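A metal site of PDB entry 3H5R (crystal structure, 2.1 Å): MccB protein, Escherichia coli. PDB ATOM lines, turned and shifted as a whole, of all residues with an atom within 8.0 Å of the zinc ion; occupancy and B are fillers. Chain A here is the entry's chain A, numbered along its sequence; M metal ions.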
ATOM      1  N   ASN A 227      -9.848  29.856  -7.325  1.00  0.00           N
ATOM      2  CA  ASN A 227     -10.523  28.984  -6.378  1.00  0.00           C
ATOM      3  C   ASN A 227      -9.776  27.663  -6.235  1.00  0.00           C
ATOM      4  O   ASN A 227      -9.364  27.341  -5.116  1.00  0.00           O
ATOM      5  CB  ASN A 227     -11.960  28.738  -6.793  1.00  0.00           C
ATOM      6  CG  ASN A 227     -12.723  27.934  -5.768  1.00  0.00           C
ATOM      7  OD1 ASN A 227     -13.000  28.420  -4.673  1.00  0.00           O
ATOM      8  ND2 ASN A 227     -13.074  26.699  -6.124  1.00  0.00           N
ATOM      9  N   VAL A 231      -7.754  26.596  -2.853  1.00  0.00           N
ATOM     10  CA  VAL A 231      -8.208  25.407  -2.113  1.00  0.00           C
ATOM     11  C   VAL A 231      -6.994  24.483  -1.902  1.00  0.00           C
ATOM     12  O   VAL A 231      -6.707  24.094  -0.759  1.00  0.00           O
ATOM     13  CB  VAL A 231      -9.404  24.661  -2.827  1.00  0.00           C
ATOM     14  CG1 VAL A 231      -9.618  23.277  -2.247  1.00  0.00           C
ATOM     15  CG2 VAL A 231     -10.686  25.471  -2.705  1.00  0.00           C
ATOM     16  N   TYR A 253     -13.386  33.022   0.832  1.00  0.00           N
ATOM     17  CA  TYR A 253     -13.065  31.630   1.018  1.00  0.00           C
ATOM     18  C   TYR A 253     -12.082  31.487   2.160  1.00  0.00           C
ATOM     19  O   TYR A 253     -11.041  32.122   2.160  1.00  0.00           O
ATOM     20  CB  TYR A 253     -12.506  31.010  -0.281  1.00  0.00           C
ATOM     21  CG  TYR A 253     -11.902  29.644  -0.071  1.00  0.00           C
ATOM     22  CD1 TYR A 253     -12.715  28.545   0.247  1.00  0.00           C
ATOM     23  CD2 TYR A 253     -10.523  29.453  -0.131  1.00  0.00           C
ATOM     24  CE1 TYR A 253     -12.148  27.286   0.460  1.00  0.00           C
ATOM     25  CE2 TYR A 253      -9.962  28.199   0.076  1.00  0.00           C
ATOM     26  CZ  TYR A 253     -10.770  27.130   0.363  1.00  0.00           C
ATOM     27  OH  TYR A 253     -10.199  25.911   0.611  1.00  0.00           O
ATOM     28  N   THR A 258     -15.215  27.466   5.174  1.00  0.00           N
ATOM     29  CA  THR A 258     -16.287  27.980   4.338  1.00  0.00           C
ATOM     30  C   THR A 258     -16.374  27.100   3.114  1.00  0.00           C
ATOM     31  O   THR A 258     -15.476  26.322   2.851  1.00  0.00           O
ATOM     32  CB  THR A 258     -15.978  29.417   3.773  1.00  0.00           C
ATOM     33  OG1 THR A 258     -14.886  29.310   2.854  1.00  0.00           O
ATOM     34  CG2 THR A 258     -15.655  30.443   4.849  1.00  0.00           C
ATOM     35  N   GLY A 259     -17.434  27.273   2.329  1.00  0.00           N
ATOM     36  CA  GLY A 259     -17.465  26.722   0.981  1.00  0.00           C
ATOM     37  C   GLY A 259     -16.523  27.451   0.020  1.00  0.00           C
ATOM     38  O   GLY A 259     -16.026  28.558   0.318  1.00  0.00           O
ATOM     39  N   CYS A 260     -16.269  26.819  -1.118  1.00  0.00           N
ATOM     40  CA  CYS A 260     -15.464  27.406  -2.169  1.00  0.00           C
ATOM     41  C   CYS A 260     -16.417  27.828  -3.270  1.00  0.00           C
ATOM     42  O   CYS A 260     -17.605  27.483  -3.250  1.00  0.00           O
ATOM     43  CB  CYS A 260     -14.419  26.399  -2.682  1.00  0.00           C
ATOM     44  SG  CYS A 260     -14.921  25.277  -4.028  1.00  0.00           S
ATOM     45  N   TYR A 261     -15.862  28.570  -4.223  1.00  0.00           N
ATOM     46  CA  TYR A 261     -16.598  29.014  -5.391  1.00  0.00           C
ATOM     47  C   TYR A 261     -17.370  27.905  -6.137  1.00  0.00           C
ATOM     48  O   TYR A 261     -18.500  28.103  -6.560  1.00  0.00           O
ATOM     49  CB  TYR A 261     -15.653  29.760  -6.339  1.00  0.00           C
ATOM     50  CG  TYR A 261     -16.364  30.684  -7.282  1.00  0.00           C
ATOM     51  CD1 TYR A 261     -16.852  31.929  -6.853  1.00  0.00           C
ATOM     52  CD2 TYR A 261     -16.580  30.311  -8.603  1.00  0.00           C
ATOM     53  CE1 TYR A 261     -17.523  32.796  -7.734  1.00  0.00           C
ATOM     54  CE2 TYR A 261     -17.243  31.156  -9.479  1.00  0.00           C
ATOM     55  CZ  TYR A 261     -17.711  32.396  -9.041  1.00  0.00           C
ATOM     56  OH  TYR A 261     -18.349  33.214  -9.954  1.00  0.00           O
ATOM     57  N   GLU A 262     -16.778  26.721  -6.243  1.00  0.00           N
ATOM     58  CA  GLU A 262     -17.359  25.673  -7.077  1.00  0.00           C
ATOM     59  C   GLU A 262     -18.350  24.793  -6.299  1.00  0.00           C
ATOM     60  O   GLU A 262     -18.896  23.842  -6.842  1.00  0.00           O
ATOM     61  CB  GLU A 262     -16.250  24.852  -7.737  1.00  0.00           C
ATOM     62  CG  GLU A 262     -15.784  25.356  -9.149  1.00  0.00           C
ATOM     63  CD  GLU A 262     -14.560  26.305  -9.126  1.00  0.00           C
ATOM     64  OE1 GLU A 262     -13.404  25.856  -8.834  1.00  0.00           O
ATOM     65  OE2 GLU A 262     -14.758  27.494  -9.437  1.00  0.00           O
ATOM     66  N   CYS A 263     -18.588  25.140  -5.023  1.00  0.00           N
ATOM     67  CA  CYS A 263     -19.361  24.297  -4.098  1.00  0.00           C
ATOM     68  C   CYS A 263     -20.843  24.116  -4.433  1.00  0.00           C
ATOM     69  O   CYS A 263     -21.352  22.991  -4.386  1.00  0.00           O
ATOM     70  CB  CYS A 263     -19.209  24.745  -2.647  1.00  0.00           C
ATOM     71  SG  CYS A 263     -18.051  23.749  -1.730  1.00  0.00           S
ATOM     72  N   GLN A 264     -21.532  25.217  -4.733  1.00  0.00           N
ATOM     73  CA  GLN A 264     -22.952  25.191  -5.095  1.00  0.00           C
ATOM     74  C   GLN A 264     -23.195  25.374  -6.620  1.00  0.00           C
ATOM     75  O   GLN A 264     -24.307  25.724  -7.043  1.00  0.00           O
ATOM     76  CB  GLN A 264     -23.740  26.211  -4.247  1.00  0.00           C
ATOM     77  CG  GLN A 264     -23.530  26.112  -2.728  1.00  0.00           C
ATOM     78  CD  GLN A 264     -24.018  24.796  -2.146  1.00  0.00           C
ATOM     79  OE1 GLN A 264     -25.076  24.298  -2.519  1.00  0.00           O
ATOM     80  NE2 GLN A 264     -23.243  24.213  -1.233  1.00  0.00           N
ATOM     81  N   LYS A 265     -22.170  25.117  -7.429  1.00  0.00           N
ATOM     82  CA  LYS A 265     -22.334  25.033  -8.872  1.00  0.00           C
ATOM     83  C   LYS A 265     -23.302  23.898  -9.231  1.00  0.00           C
ATOM     84  O   LYS A 265     -23.034  22.715  -8.942  1.00  0.00           O
ATOM     85  CB  LYS A 265     -20.982  24.843  -9.575  1.00  0.00           C
ATOM     86  N   MET A 340     -23.167  29.881  -0.923  1.00  0.00           N
ATOM     87  CA  MET A 340     -21.953  29.285  -1.410  1.00  0.00           C
ATOM     88  C   MET A 340     -21.301  28.534  -0.266  1.00  0.00           C
ATOM     89  O   MET A 340     -20.087  28.577  -0.084  1.00  0.00           O
ATOM     90  CB  MET A 340     -21.048  30.376  -1.971  1.00  0.00           C
ATOM     91  CG  MET A 340     -21.521  30.848  -3.308  1.00  0.00           C
ATOM     92  SD  MET A 340     -20.213  31.516  -4.352  1.00  0.00           S
ATOM     93  CE  MET A 340     -18.797  30.715  -3.634  1.00  0.00           C
ATOM     94  N   GLY A 341     -22.134  27.868   0.521  1.00  0.00           N
ATOM     95  CA  GLY A 341     -21.659  27.121   1.675  1.00  0.00           C
ATOM     96  C   GLY A 341     -21.053  25.799   1.233  1.00  0.00           C
ATOM     97  O   GLY A 341     -21.176  25.424   0.075  1.00  0.00           O
ATOM     98  N   ARG A 342     -20.405  25.102   2.164  1.00  0.00           N
ATOM     99  CA  ARG A 342     -19.624  23.900   1.837  1.00  0.00           C
ATOM    100  C   ARG A 342     -20.513  22.755   1.394  1.00  0.00           C
ATOM    101  O   ARG A 342     -21.465  22.400   2.097  1.00  0.00           O
ATOM    102  CB  ARG A 342     -18.764  23.464   3.033  1.00  0.00           C
ATOM    103  CG  ARG A 342     -17.559  22.605   2.662  1.00  0.00           C
ATOM    104  CD  ARG A 342     -16.627  22.371   3.865  1.00  0.00           C
ATOM    105  NE  ARG A 342     -15.542  21.445   3.531  1.00  0.00           N
ATOM    106  CZ  ARG A 342     -14.723  20.860   4.408  1.00  0.00           C
ATOM    107  NH1 ARG A 342     -14.836  21.106   5.714  1.00  0.00           N
ATOM    108  NH2 ARG A 342     -13.776  20.030   3.983  1.00  0.00           N
ATOM    109  N   SER A 343     -20.195  22.186   0.243  1.00  0.00           N
ATOM    110  CA  SER A 343     -20.756  20.907  -0.166  1.00  0.00           C
ATOM    111  C   SER A 343     -19.678  19.824  -0.045  1.00  0.00           C
ATOM    112  O   SER A 343     -18.596  19.950  -0.616  1.00  0.00           O
ATOM    113  CB  SER A 343     -21.328  20.944  -1.581  1.00  0.00           C
ATOM    114  OG  SER A 343     -21.884  19.671  -1.918  1.00  0.00           O
ATOM    115  N   PRO A 344     -19.984  18.779   0.737  1.00  0.00           N
ATOM    116  CA  PRO A 344     -19.056  17.689   1.008  1.00  0.00           C
ATOM    117  C   PRO A 344     -18.833  16.900  -0.267  1.00  0.00           C
ATOM    118  O   PRO A 344     -17.815  16.216  -0.412  1.00  0.00           O
ATOM    119  CB  PRO A 344     -19.804  16.840   2.044  1.00  0.00           C
ATOM    120  CG  PRO A 344     -21.241  17.135   1.817  1.00  0.00           C
ATOM    121  CD  PRO A 344     -21.284  18.584   1.420  1.00  0.00           C
ATOM    122  N   VAL A 345     -19.787  17.043  -1.189  1.00  0.00           N
ATOM    123  CA  VAL A 345     -19.763  16.426  -2.500  1.00  0.00           C
ATOM    124  C   VAL A 345     -18.968  17.272  -3.521  1.00  0.00           C
ATOM    125  O   VAL A 345     -18.690  16.815  -4.623  1.00  0.00           O
ATOM    126  CB  VAL A 345     -21.222  16.097  -2.952  1.00  0.00           C
ATOM    127  CG1 VAL A 345     -21.452  16.293  -4.444  1.00  0.00           C
ATOM    128  CG2 VAL A 345     -21.606  14.686  -2.512  1.00  0.00           C
ATOM    129  N   CYS A 346     -18.568  18.488  -3.150  1.00  0.00           N
ATOM    130  CA  CYS A 346     -17.856  19.362  -4.101  1.00  0.00           C
ATOM    131  C   CYS A 346     -16.690  18.678  -4.765  1.00  0.00           C
ATOM    132  O   CYS A 346     -15.962  17.882  -4.154  1.00  0.00           O
ATOM    133  CB  CYS A 346     -17.367  20.655  -3.448  1.00  0.00           C
ATOM    134  SG  CYS A 346     -16.349  21.675  -4.538  1.00  0.00           S
ATOM    135  N   SER A 347     -16.534  19.008  -6.043  1.00  0.00           N
ATOM    136  CA  SER A 347     -15.498  18.492  -6.920  1.00  0.00           C
ATOM    137  C   SER A 347     -14.129  19.024  -6.546  1.00  0.00           C
ATOM    138  O   SER A 347     -13.113  18.363  -6.757  1.00  0.00           O
ATOM    139  CB  SER A 347     -15.822  18.912  -8.355  1.00  0.00           C
ATOM    140  OG  SER A 347     -14.672  18.802  -9.181  1.00  0.00           O
ATOM    141  N   VAL A 348     -14.110  20.239  -6.006  1.00  0.00           N
ATOM    142  CA  VAL A 348     -12.889  20.982  -5.781  1.00  0.00           C
ATOM    143  C   VAL A 348     -12.384  20.807  -4.351  1.00  0.00           C
ATOM    144  O   VAL A 348     -11.254  20.334  -4.162  1.00  0.00           O
ATOM    145  CB  VAL A 348     -13.081  22.461  -6.140  1.00  0.00           C
ATOM    146  CG1 VAL A 348     -11.884  23.281  -5.738  1.00  0.00           C
ATOM    147  CG2 VAL A 348     -13.336  22.591  -7.631  1.00  0.00           C
ATOM    148  N   CYS A 349     -13.205  21.163  -3.355  1.00  0.00           N
ATOM    149  CA  CYS A 349     -12.760  21.071  -1.974  1.00  0.00           C
ATOM    150  C   CYS A 349     -13.308  19.864  -1.197  1.00  0.00           C
ATOM    151  O   CYS A 349     -13.030  19.728   0.006  1.00  0.00           O
ATOM    152  CB  CYS A 349     -13.076  22.370  -1.236  1.00  0.00           C
ATOM    153  SG  CYS A 349     -14.835  22.659  -1.038  1.00  0.00           S
ATOM    154  N   GLY A 350     -14.055  18.992  -1.863  1.00  0.00           N
ATOM    155  CA  GLY A 350     -14.802  17.934  -1.181  1.00  0.00           C
ATOM    156  C   GLY A 350     -13.994  16.675  -0.976  1.00  0.00           C
ATOM    157  O   GLY A 350     -12.798  16.659  -1.270  1.00  0.00           O
HETATM  158 ZN    ZN M   1     -15.994  23.408  -2.892  1.00  0.00          ZN
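SG of Cys 263 lies close to N of Ser 343 (3.3 Å). SG of Cys 346 lies close to N of Val 348, 3.0 Å away. The side-chain sulfur (SG) of Cys 260 sits close to the backbone NH (N) of Glu 262 (3.2 Å). The side-chain sulfur (SG) of Cys 260 lies close to the side-chain amide nitrogen (ND2) of Asn 227 (3.1 Å).
Within 4 Å of the zinc ion: Cys 260, Cys 263, Cys 346 and Cys 349.
The zinc ion is bound by the side-chain sulfur of Cys 349, the side-chain sulfur of Cys 263, the side-chain sulfur of Cys 346 and the side-chain sulfur of Cys 260.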
